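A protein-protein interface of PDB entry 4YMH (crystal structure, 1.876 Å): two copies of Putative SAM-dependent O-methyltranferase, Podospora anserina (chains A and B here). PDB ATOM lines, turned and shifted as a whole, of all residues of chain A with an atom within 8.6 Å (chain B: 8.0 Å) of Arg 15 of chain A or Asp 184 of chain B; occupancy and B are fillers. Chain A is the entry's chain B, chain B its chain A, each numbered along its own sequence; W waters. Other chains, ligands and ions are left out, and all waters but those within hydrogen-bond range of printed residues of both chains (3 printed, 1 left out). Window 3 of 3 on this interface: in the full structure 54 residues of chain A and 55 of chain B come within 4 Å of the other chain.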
ATOM      1  N   PHE A   8      27.340 -29.824   5.963  1.00  0.00           N
ATOM      2  CA  PHE A   8      27.992 -28.796   6.787  1.00  0.00           C
ATOM      3  C   PHE A   8      28.652 -27.747   5.900  1.00  0.00           C
ATOM      4  O   PHE A   8      29.161 -28.086   4.834  1.00  0.00           O
ATOM      5  CB  PHE A   8      29.063 -29.407   7.688  1.00  0.00           C
ATOM      6  CG  PHE A   8      28.540 -30.360   8.720  1.00  0.00           C
ATOM      7  CD1 PHE A   8      27.684 -29.923   9.717  1.00  0.00           C
ATOM      8  CD2 PHE A   8      28.952 -31.682   8.726  1.00  0.00           C
ATOM      9  CE1 PHE A   8      27.215 -30.797  10.680  1.00  0.00           C
ATOM     10  CE2 PHE A   8      28.490 -32.558   9.694  1.00  0.00           C
ATOM     11  CZ  PHE A   8      27.619 -32.114  10.666  1.00  0.00           C
ATOM     12  N   ASN A   9      28.684 -26.485   6.324  1.00  0.00           N
ATOM     13  CA  ASN A   9      29.552 -25.535   5.618  1.00  0.00           C
ATOM     14  C   ASN A   9      30.976 -25.704   6.164  1.00  0.00           C
ATOM     15  O   ASN A   9      31.203 -26.540   7.044  1.00  0.00           O
ATOM     16  CB  ASN A   9      29.048 -24.077   5.722  1.00  0.00           C
ATOM     17  CG  ASN A   9      28.906 -23.580   7.152  1.00  0.00           C
ATOM     18  OD1 ASN A   9      29.522 -24.100   8.078  1.00  0.00           O
ATOM     19  ND2 ASN A   9      28.098 -22.539   7.329  1.00  0.00           N
ATOM     20  N   GLU A  10      31.939 -24.962   5.621  1.00  0.00           N
ATOM     21  CA  GLU A  10      33.350 -25.154   5.997  1.00  0.00           C
ATOM     22  C   GLU A  10      33.592 -24.970   7.504  1.00  0.00           C
ATOM     23  O   GLU A  10      34.187 -25.832   8.165  1.00  0.00           O
ATOM     24  CB  GLU A  10      34.245 -24.179   5.224  1.00  0.00           C
ATOM     25  CG  GLU A  10      34.147 -24.330   3.714  1.00  0.00           C
ATOM     26  CD  GLU A  10      34.863 -23.228   2.962  1.00  0.00           C
ATOM     27  OE1 GLU A  10      34.167 -22.359   2.390  1.00  0.00           O
ATOM     28  OE2 GLU A  10      36.117 -23.238   2.924  1.00  0.00           O
ATOM     29  N   GLU A  11      33.103 -23.845   8.034  1.00  0.00           N
ATOM     30  CA  GLU A  11      33.322 -23.513   9.442  1.00  0.00           C
ATOM     31  C   GLU A  11      32.766 -24.604  10.346  1.00  0.00           C
ATOM     32  O   GLU A  11      33.428 -25.069  11.287  1.00  0.00           O
ATOM     33  CB  GLU A  11      32.684 -22.158   9.795  1.00  0.00           C
ATOM     34  CG  GLU A  11      32.991 -21.690  11.201  1.00  0.00           C
ATOM     35  CD  GLU A  11      32.044 -20.592  11.670  1.00  0.00           C
ATOM     36  OE1 GLU A  11      31.214 -20.131  10.857  1.00  0.00           O
ATOM     37  OE2 GLU A  11      32.127 -20.198  12.853  1.00  0.00           O
ATOM     38  N   THR A  12      31.555 -25.039  10.028  1.00  0.00           N
ATOM     39  CA  THR A  12      30.880 -26.057  10.824  1.00  0.00           C
ATOM     40  C   THR A  12      31.514 -27.439  10.662  1.00  0.00           C
ATOM     41  O   THR A  12      31.649 -28.171  11.633  1.00  0.00           O
ATOM     42  CB  THR A  12      29.388 -26.148  10.461  1.00  0.00           C
ATOM     43  OG1 THR A  12      28.808 -24.839  10.520  1.00  0.00           O
ATOM     44  CG2 THR A  12      28.669 -27.068  11.431  1.00  0.00           C
ATOM     45  N   ALA A  13      31.900 -27.809   9.445  1.00  0.00           N
ATOM     46  CA  ALA A  13      32.650 -29.061   9.276  1.00  0.00           C
ATOM     47  C   ALA A  13      33.876 -29.062  10.196  1.00  0.00           C
ATOM     48  O   ALA A  13      34.188 -30.068  10.863  1.00  0.00           O
ATOM     49  CB  ALA A  13      33.083 -29.244   7.818  1.00  0.00           C
ATOM     50  N   ASP A  14      34.575 -27.935  10.230  1.00  0.00           N
ATOM     51  CA  ASP A  14      35.778 -27.869  11.058  1.00  0.00           C
ATOM     52  C   ASP A  14      35.433 -27.962  12.551  1.00  0.00           C
ATOM     53  O   ASP A  14      36.143 -28.622  13.325  1.00  0.00           O
ATOM     54  CB  ASP A  14      36.578 -26.601  10.745  1.00  0.00           C
ATOM     55  CG  ASP A  14      37.444 -26.765   9.495  1.00  0.00           C
ATOM     56  OD1 ASP A  14      37.499 -27.900   8.956  1.00  0.00           O
ATOM     57  OD2 ASP A  14      38.080 -25.782   9.064  1.00  0.00           O
ATOM     58  N   ARG A  15      34.347 -27.310  12.967  1.00  0.00           N
ATOM     59  CA  ARG A  15      33.912 -27.451  14.366  1.00  0.00           C
ATOM     60  C   ARG A  15      33.560 -28.904  14.743  1.00  0.00           C
ATOM     61  O   ARG A  15      33.885 -29.390  15.836  1.00  0.00           O
ATOM     62  CB  ARG A  15      32.696 -26.554  14.637  1.00  0.00           C
ATOM     63  CG  ARG A  15      33.056 -25.122  14.896  1.00  0.00           C
ATOM     64  CD  ARG A  15      31.791 -24.254  14.931  1.00  0.00           C
ATOM     65  NE  ARG A  15      30.963 -24.500  16.107  1.00  0.00           N
ATOM     66  CZ  ARG A  15      29.782 -23.922  16.304  1.00  0.00           C
ATOM     67  NH1 ARG A  15      29.291 -23.108  15.383  1.00  0.00           N
ATOM     68  NH2 ARG A  15      29.097 -24.153  17.415  1.00  0.00           N
ATOM     69  N   VAL A  16      32.875 -29.598  13.842  1.00  0.00           N
ATOM     70  CA  VAL A  16      32.460 -30.962  14.135  1.00  0.00           C
ATOM     71  C   VAL A  16      33.674 -31.882  14.173  1.00  0.00           C
ATOM     72  O   VAL A  16      33.771 -32.752  15.034  1.00  0.00           O
ATOM     73  CB  VAL A  16      31.425 -31.475  13.111  1.00  0.00           C
ATOM     74  CG1 VAL A  16      31.082 -32.929  13.396  1.00  0.00           C
ATOM     75  CG2 VAL A  16      30.157 -30.592  13.184  1.00  0.00           C
ATOM     76  N   SER A  17      34.619 -31.659  13.265  1.00  0.00           N
ATOM     77  CA  SER A  17      35.859 -32.422  13.278  1.00  0.00           C
ATOM     78  C   SER A  17      36.638 -32.200  14.593  1.00  0.00           C
ATOM     79  O   SER A  17      37.116 -33.163  15.228  1.00  0.00           O
ATOM     80  CB  SER A  17      36.709 -32.054  12.057  1.00  0.00           C
ATOM     81  OG  SER A  17      37.909 -32.797  12.040  1.00  0.00           O
ATOM     82  N   ALA A  18      36.728 -30.943  15.033  1.00  0.00           N
ATOM     83  CA  ALA A  18      37.395 -30.673  16.315  1.00  0.00           C
ATOM     84  C   ALA A  18      36.677 -31.376  17.476  1.00  0.00           C
ATOM     85  O   ALA A  18      37.312 -31.860  18.428  1.00  0.00           O
ATOM     86  CB  ALA A  18      37.476 -29.165  16.576  1.00  0.00           C
ATOM     87  N   TYR A  19      35.352 -31.406  17.399  1.00  0.00           N
ATOM     88  CA  TYR A  19      34.552 -32.076  18.427  1.00  0.00           C
ATOM     89  C   TYR A  19      34.832 -33.586  18.453  1.00  0.00           C
ATOM     90  O   TYR A  19      34.939 -34.193  19.529  1.00  0.00           O
ATOM     91  CB  TYR A  19      33.060 -31.825  18.199  1.00  0.00           C
ATOM     92  CG  TYR A  19      32.173 -32.384  19.290  1.00  0.00           C
ATOM     93  CD1 TYR A  19      31.864 -31.631  20.407  1.00  0.00           C
ATOM     94  CD2 TYR A  19      31.639 -33.668  19.195  1.00  0.00           C
ATOM     95  CE1 TYR A  19      31.043 -32.140  21.415  1.00  0.00           C
ATOM     96  CE2 TYR A  19      30.830 -34.182  20.195  1.00  0.00           C
ATOM     97  CZ  TYR A  19      30.538 -33.417  21.298  1.00  0.00           C
ATOM     98  OH  TYR A  19      29.749 -33.927  22.300  1.00  0.00           O
ATOM     99  N   CYS A  20      34.937 -34.192  17.278  1.00  0.00           N
ATOM    100  CA  CYS A  20      35.294 -35.615  17.188  1.00  0.00           C
ATOM    101  C   CYS A  20      36.661 -35.889  17.765  1.00  0.00           C
ATOM    102  O   CYS A  20      36.867 -36.913  18.416  1.00  0.00           O
ATOM    103  CB  CYS A  20      35.265 -36.095  15.744  1.00  0.00           C
ATOM    104  SG  CYS A  20      33.576 -36.169  15.068  1.00  0.00           S
ATOM    105  N   GLU A  21      37.585 -34.978  17.596  1.00  0.00           N
ATOM    106  CA  GLU A  21      38.920 -35.138  18.112  1.00  0.00           C
ATOM    107  C   GLU A  21      38.918 -35.075  19.596  1.00  0.00           C
ATOM    108  O   GLU A  21      39.566 -35.809  20.251  1.00  0.00           O
ATOM    109  CB  GLU A  21      39.775 -34.005  17.647  1.00  0.00           C
ATOM    110  CG  GLU A  21      40.424 -34.173  16.328  1.00  0.00           C
ATOM    111  CD  GLU A  21      41.473 -33.089  16.064  1.00  0.00           C
ATOM    112  OE1 GLU A  21      42.438 -32.969  16.787  1.00  0.00           O
ATOM    113  OE2 GLU A  21      41.260 -32.356  15.151  1.00  0.00           O
ATOM    114  N   LYS A  22      38.197 -34.113  20.109  1.00  0.00           N
ATOM    115  CA  LYS A  22      38.099 -33.927  21.550  1.00  0.00           C
ATOM    116  C   LYS A  22      37.440 -35.128  22.225  1.00  0.00           C
ATOM    117  O   LYS A  22      37.770 -35.473  23.349  1.00  0.00           O
ATOM    118  CB  LYS A  22      37.309 -32.649  21.868  1.00  0.00           C
ATOM    119  CG  LYS A  22      37.244 -32.285  23.349  1.00  0.00           C
ATOM    120  CD  LYS A  22      36.652 -30.891  23.517  1.00  0.00           C
ATOM    121  CE  LYS A  22      36.509 -30.491  24.982  1.00  0.00           C
ATOM    122  NZ  LYS A  22      35.454 -31.270  25.684  1.00  0.00           N
ATOM    123  N   ASN A  23      36.515 -35.774  21.528  1.00  0.00           N
ATOM    124  CA  ASN A  23      35.758 -36.863  22.127  1.00  0.00           C
ATOM    125  C   ASN A  23      36.141 -38.250  21.599  1.00  0.00           C
ATOM    126  O   ASN A  23      35.338 -39.183  21.609  1.00  0.00           O
ATOM    127  CB  ASN A  23      34.276 -36.585  21.933  1.00  0.00           C
ATOM    128  CG  ASN A  23      33.812 -35.396  22.790  1.00  0.00           C
ATOM    129  OD1 ASN A  23      33.586 -35.552  23.973  1.00  0.00           O
ATOM    130  ND2 ASN A  23      33.735 -34.208  22.200  1.00  0.00           N
ATOM    131  N   LEU B   2      42.461 -26.868   9.964  1.00  0.00           N
ATOM    132  CA  LEU B   2      41.282 -27.420   9.308  1.00  0.00           C
ATOM    133  C   LEU B   2      41.230 -28.926   9.578  1.00  0.00           C
ATOM    134  O   LEU B   2      42.257 -29.552   9.852  1.00  0.00           O
ATOM    135  CB  LEU B   2      41.303 -27.105   7.801  1.00  0.00           C
ATOM    136  CG  LEU B   2      40.335 -27.790   6.834  1.00  0.00           C
ATOM    137  CD1 LEU B   2      39.840 -26.787   5.813  1.00  0.00           C
ATOM    138  CD2 LEU B   2      40.986 -28.972   6.133  1.00  0.00           C
ATOM    139  N   GLY B   3      40.037 -29.504   9.506  1.00  0.00           N
ATOM    140  CA  GLY B   3      39.838 -30.860   9.974  1.00  0.00           C
ATOM    141  C   GLY B   3      39.613 -31.951   8.949  1.00  0.00           C
ATOM    142  O   GLY B   3      40.080 -31.890   7.810  1.00  0.00           O
ATOM    143  N   ILE B   5      36.548 -33.400   7.944  1.00  0.00           N
ATOM    144  CA  ILE B   5      35.223 -33.563   7.359  1.00  0.00           C
ATOM    145  C   ILE B   5      35.020 -32.691   6.120  1.00  0.00           C
ATOM    146  O   ILE B   5      35.306 -31.502   6.139  1.00  0.00           O
ATOM    147  CB  ILE B   5      34.137 -33.233   8.415  1.00  0.00           C
ATOM    148  CG1 ILE B   5      34.248 -34.209   9.587  1.00  0.00           C
ATOM    149  CG2 ILE B   5      32.740 -33.245   7.821  1.00  0.00           C
ATOM    150  CD1 ILE B   5      33.409 -33.795  10.783  1.00  0.00           C
ATOM    151  N   ARG B 177      22.078 -34.794  14.292  1.00  0.00           N
ATOM    152  CA  ARG B 177      22.001 -33.943  13.100  1.00  0.00           C
ATOM    153  C   ARG B 177      23.025 -32.808  13.089  1.00  0.00           C
ATOM    154  O   ARG B 177      22.994 -31.940  12.209  1.00  0.00           O
ATOM    155  CB  ARG B 177      20.585 -33.374  12.959  1.00  0.00           C
ATOM    156  CG  ARG B 177      19.488 -34.438  13.008  1.00  0.00           C
ATOM    157  CD  ARG B 177      19.565 -35.347  11.809  1.00  0.00           C
ATOM    158  NE  ARG B 177      18.279 -35.997  11.554  1.00  0.00           N
ATOM    159  CZ  ARG B 177      17.992 -37.263  11.844  1.00  0.00           C
ATOM    160  NH1 ARG B 177      18.902 -38.051  12.401  1.00  0.00           N
ATOM    161  NH2 ARG B 177      16.785 -37.745  11.561  1.00  0.00           N
ATOM    162  N   GLY B 178      23.933 -32.822  14.059  1.00  0.00           N
ATOM    163  CA  GLY B 178      24.912 -31.767  14.228  1.00  0.00           C
ATOM    164  C   GLY B 178      24.694 -31.026  15.535  1.00  0.00           C
ATOM    165  O   GLY B 178      25.581 -30.356  16.032  1.00  0.00           O
ATOM    166  N   LEU B 179      23.516 -31.182  16.128  1.00  0.00           N
ATOM    167  CA  LEU B 179      23.179 -30.366  17.292  1.00  0.00           C
ATOM    168  C   LEU B 179      23.877 -30.818  18.578  1.00  0.00           C
ATOM    169  O   LEU B 179      23.944 -30.047  19.553  1.00  0.00           O
ATOM    170  CB  LEU B 179      21.657 -30.336  17.493  1.00  0.00           C
ATOM    171  CG  LEU B 179      20.851 -29.767  16.314  1.00  0.00           C
ATOM    172  CD1 LEU B 179      19.368 -29.596  16.707  1.00  0.00           C
ATOM    173  CD2 LEU B 179      21.426 -28.447  15.826  1.00  0.00           C
ATOM    174  N   THR B 180      24.424 -32.033  18.582  1.00  0.00           N
ATOM    175  CA  THR B 180      25.279 -32.467  19.694  1.00  0.00           C
ATOM    176  C   THR B 180      26.486 -31.543  19.838  1.00  0.00           C
ATOM    177  O   THR B 180      26.922 -31.212  20.950  1.00  0.00           O
ATOM    178  CB  THR B 180      25.771 -33.927  19.495  1.00  0.00           C
ATOM    179  OG1 THR B 180      24.652 -34.815  19.583  1.00  0.00           O
ATOM    180  CG2 THR B 180      26.798 -34.304  20.551  1.00  0.00           C
ATOM    181  N   ILE B 181      27.021 -31.105  18.706  1.00  0.00           N
ATOM    182  CA  ILE B 181      28.198 -30.243  18.719  1.00  0.00           C
ATOM    183  C   ILE B 181      27.819 -28.813  19.151  1.00  0.00           C
ATOM    184  O   ILE B 181      28.511 -28.174  19.941  1.00  0.00           O
ATOM    185  CB  ILE B 181      28.906 -30.236  17.336  1.00  0.00           C
ATOM    186  CG1 ILE B 181      29.377 -31.642  16.965  1.00  0.00           C
ATOM    187  CG2 ILE B 181      30.117 -29.282  17.362  1.00  0.00           C
ATOM    188  CD1 ILE B 181      28.306 -32.524  16.285  1.00  0.00           C
ATOM    189  N   GLY B 182      26.697 -28.315  18.658  1.00  0.00           N
ATOM    190  CA  GLY B 182      26.210 -27.003  19.092  1.00  0.00           C
ATOM    191  C   GLY B 182      24.870 -26.728  18.462  1.00  0.00           C
ATOM    192  O   GLY B 182      24.565 -27.272  17.403  1.00  0.00           O
ATOM    193  N   PRO B 183      24.050 -25.881  19.099  1.00  0.00           N
ATOM    194  CA  PRO B 183      22.700 -25.677  18.575  1.00  0.00           C
ATOM    195  C   PRO B 183      22.682 -24.968  17.225  1.00  0.00           C
ATOM    196  O   PRO B 183      21.643 -25.026  16.556  1.00  0.00           O
ATOM    197  CB  PRO B 183      22.032 -24.812  19.658  1.00  0.00           C
ATOM    198  CG  PRO B 183      23.174 -24.106  20.313  1.00  0.00           C
ATOM    199  CD  PRO B 183      24.283 -25.121  20.340  1.00  0.00           C
ATOM    200  N   ASP B 184      23.794 -24.328  16.843  1.00  0.00           N
ATOM    201  CA  ASP B 184      23.892 -23.622  15.561  1.00  0.00           C
ATOM    202  C   ASP B 184      24.527 -24.457  14.441  1.00  0.00           C
ATOM    203  O   ASP B 184      24.824 -23.934  13.370  1.00  0.00           O
ATOM    204  CB  ASP B 184      24.684 -22.316  15.724  1.00  0.00           C
ATOM    205  CG  ASP B 184      26.119 -22.533  16.191  1.00  0.00           C
ATOM    206  OD1 ASP B 184      26.386 -23.470  16.978  1.00  0.00           O
ATOM    207  OD2 ASP B 184      26.988 -21.732  15.784  1.00  0.00           O
ATOM    208  N   CYS B 185      24.680 -25.757  14.658  1.00  0.00           N
ATOM    209  CA  CYS B 185      25.436 -26.570  13.710  1.00  0.00           C
ATOM    210  C   CYS B 185      24.573 -27.293  12.662  1.00  0.00           C
ATOM    211  O   CYS B 185      25.092 -28.099  11.892  1.00  0.00           O
ATOM    212  CB  CYS B 185      26.290 -27.586  14.475  1.00  0.00           C
ATOM    213  SG  CYS B 185      27.701 -26.839  15.350  1.00  0.00           S
ATOM    214  N   ALA B 186      23.276 -26.993  12.621  1.00  0.00           N
ATOM    215  CA  ALA B 186      22.411 -27.595  11.608  1.00  0.00           C
ATOM    216  C   ALA B 186      21.343 -26.628  11.118  1.00  0.00           C
ATOM    217  O   ALA B 186      20.157 -26.867  11.340  1.00  0.00           O
ATOM    218  CB  ALA B 186      21.759 -28.861  12.159  1.00  0.00           C
ATOM    219  N   PRO B 187      21.755 -25.540  10.436  1.00  0.00           N
ATOM    220  CA  PRO B 187      20.794 -24.492  10.073  1.00  0.00           C
ATOM    221  C   PRO B 187      19.775 -24.974   9.043  1.00  0.00           C
ATOM    222  O   PRO B 187      18.696 -24.390   8.956  1.00  0.00           O
ATOM    223  CB  PRO B 187      21.680 -23.363   9.519  1.00  0.00           C
ATOM    224  CG  PRO B 187      22.958 -24.021   9.136  1.00  0.00           C
ATOM    225  CD  PRO B 187      23.137 -25.199  10.054  1.00  0.00           C
ATOM    226  N   TRP B 188      20.111 -26.036   8.309  1.00  0.00           N
ATOM    227  CA  TRP B 188      19.227 -26.631   7.301  1.00  0.00           C
ATOM    228  C   TRP B 188      18.067 -27.391   7.929  1.00  0.00           C
ATOM    229  O   TRP B 188      17.070 -27.670   7.260  1.00  0.00           O
ATOM    230  CB  TRP B 188      20.022 -27.597   6.397  1.00  0.00           C
ATOM    231  CG  TRP B 188      20.719 -28.648   7.207  1.00  0.00           C
ATOM    232  CD1 TRP B 188      21.961 -28.553   7.782  1.00  0.00           C
ATOM    233  CD2 TRP B 188      20.207 -29.937   7.575  1.00  0.00           C
ATOM    234  NE1 TRP B 188      22.248 -29.706   8.478  1.00  0.00           N
ATOM    235  CE2 TRP B 188      21.189 -30.570   8.364  1.00  0.00           C
ATOM    236  CE3 TRP B 188      19.012 -30.618   7.312  1.00  0.00           C
ATOM    237  CZ2 TRP B 188      21.016 -31.848   8.888  1.00  0.00           C
ATOM    238  CZ3 TRP B 188      18.844 -31.887   7.830  1.00  0.00           C
ATOM    239  CH2 TRP B 188      19.837 -32.487   8.613  1.00  0.00           C
ATOM    240  N   ARG B 194      13.463 -29.442  15.478  1.00  0.00           N
ATOM    241  CA  ARG B 194      14.646 -28.842  16.104  1.00  0.00           C
ATOM    242  C   ARG B 194      14.660 -28.970  17.651  1.00  0.00           C
ATOM    243  O   ARG B 194      15.667 -29.389  18.215  1.00  0.00           O
ATOM    244  CB  ARG B 194      14.756 -27.375  15.659  1.00  0.00           C
ATOM    245  CG  ARG B 194      16.028 -26.654  16.045  1.00  0.00           C
ATOM    246  CD  ARG B 194      16.109 -25.263  15.366  1.00  0.00           C
ATOM    247  NE  ARG B 194      16.342 -25.337  13.915  1.00  0.00           N
ATOM    248  CZ  ARG B 194      17.539 -25.531  13.361  1.00  0.00           C
ATOM    249  NH1 ARG B 194      18.602 -25.712  14.131  1.00  0.00           N
ATOM    250  NH2 ARG B 194      17.676 -25.575  12.040  1.00  0.00           N
ATOM    251  N   ASN B 198      17.637 -30.954  19.619  1.00  0.00           N
ATOM    252  CA  ASN B 198      18.481 -30.180  20.526  1.00  0.00           C
ATOM    253  C   ASN B 198      18.558 -30.865  21.883  1.00  0.00           C
ATOM    254  O   ASN B 198      19.626 -30.929  22.502  1.00  0.00           O
ATOM    255  CB  ASN B 198      17.942 -28.752  20.687  1.00  0.00           C
ATOM    256  CG  ASN B 198      18.655 -27.754  19.793  1.00  0.00           C
ATOM    257  OD1 ASN B 198      19.890 -27.674  19.777  1.00  0.00           O
ATOM    258  ND2 ASN B 198      17.880 -26.997  19.030  1.00  0.00           N
HETATM  259  O   HOH W   1      29.698 -25.777  19.688  1.00  0.00           O
HETATM  260  O   HOH W   2      39.141 -28.961  12.794  1.00  0.00           O
HETATM  261  O   HOH W   3      26.252 -23.954  11.025  1.00  0.00           O
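The side-chain amide nitrogen of Asn 23 of chain A sits at hydrogen-bond distance from the backbone carbonyl oxygen of Tyr 19 of chain A, 2.9 Å away. The backbone carbonyl oxygen (O) of Val 16 of chain A lies within hydrogen-bond range of the side-chain sulfur (SG) of Cys 20 of chain A, at 3.4 Å. OG1 of Thr 12 of chain A is in hydrogen-bond range of OD1 of Asn 9 of chain A, 2.6 Å away. N of Gly 182 of chain B lies within hydrogen-bond range of SG of Cys 185 of chain B, at 3.8 Å.
Of the printed residues of chain B, Asp 14 of chain A touches Leu 2 (3.5 Å) and Gly 3 (3.1 Å). Arg 15 of chain A touches just these residues of chain B: Asp 184 and Cys 185. Printed residues of chain B within 4 Å of Ser 17 of chain A: Gly 3 (3.4 Å) and Ile 5 (3.5 Å). Printed residues of chain A within 4 Å of Gly 3 of chain B: Asp 14 and Ser 17. Pro 183 of chain B touches none of the printed residues of chain A. Of chain A, only Arg 15 comes within 4 Å of Asp 184 of chain B. The nearest residue of chain B that does not touch Arg 15 of chain A is Ile 181 of chain B (4.1 Å). The nearest residue of chain A that does not touch Asp 184 of chain B is Thr 12 of chain A (5.0 Å).
OD2 of Asp 184 of chain B is in salt-bridge range of NH1 of Arg 15 of chain A (2.7 Å). N of Gly 3 of chain B lies within hydrogen-bond range of OD1 of Asp 14 of chain A. SG of Cys 185 of chain B lies within hydrogen-bond range of NH2 of Arg 15 of chain A, at 3.7 Å.
Water W1 bridges O of Ile 181 of chain B (2.7 Å) and NH2 of Arg 15 of chain A (2.9 Å). Water W3 bridges the backbone carbonyl oxygen (O) of Asp 184 of chain B (2.7 Å) and the side-chain hydroxyl (OG1) of Thr 12 of chain A (2.8 Å). Water W2 lies within hydrogen-bond range of O of Asp 14 of chain A (3.1 Å) and N of Gly 3 of chain B (3.5 Å).
Printed residues of chain B that touch a printed residue of chain A: Leu 2, Gly 3, Ile 5, Thr 180, Ile 181, Asp 184 and Cys 185. Hydrophobic or aromatic side chains of chain B within 4 Å of the printed part of chain A: Leu 2, Ile 5 and Ile 181. Of the 16 printed residues of chain A, 8 touch a printed residue of chain B. Hydrophobic or aromatic side chains of chain A that line the printed part of chain B: Phe 8, Ala 13, Val 16 and Tyr 19. Among the printed residues, Asp or Glu carboxylates within 4 Å of a Lys or Arg side-chain nitrogen of the other chain: Arg 15 of chain A with Asp 184 of chain B.
No position is printed for both chains.
Among the printed residues, pairs that only touch across the chains: Ser 17 of chain A with Gly 3 of chain B (3.4 Å), Tyr 19 of chain A with Thr 180 of chain B (3.5 Å), Ser 17 of chain A with Ile 5 of chain B (3.5 Å), Asp 14 of chain A with Leu 2 of chain B (3.5 Å), Ala 13 of chain A with Ile 5 of chain B (3.6 Å), Val 16 of chain A with Ile 5 of chain B (3.6 Å), Phe 8 of chain A with Cys 185 of chain B (3.6 Å), Tyr 19 of chain A with Ile 181 of chain B (3.7 Å) and Thr 12 of chain A with Cys 185 of chain B (3.8 Å).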
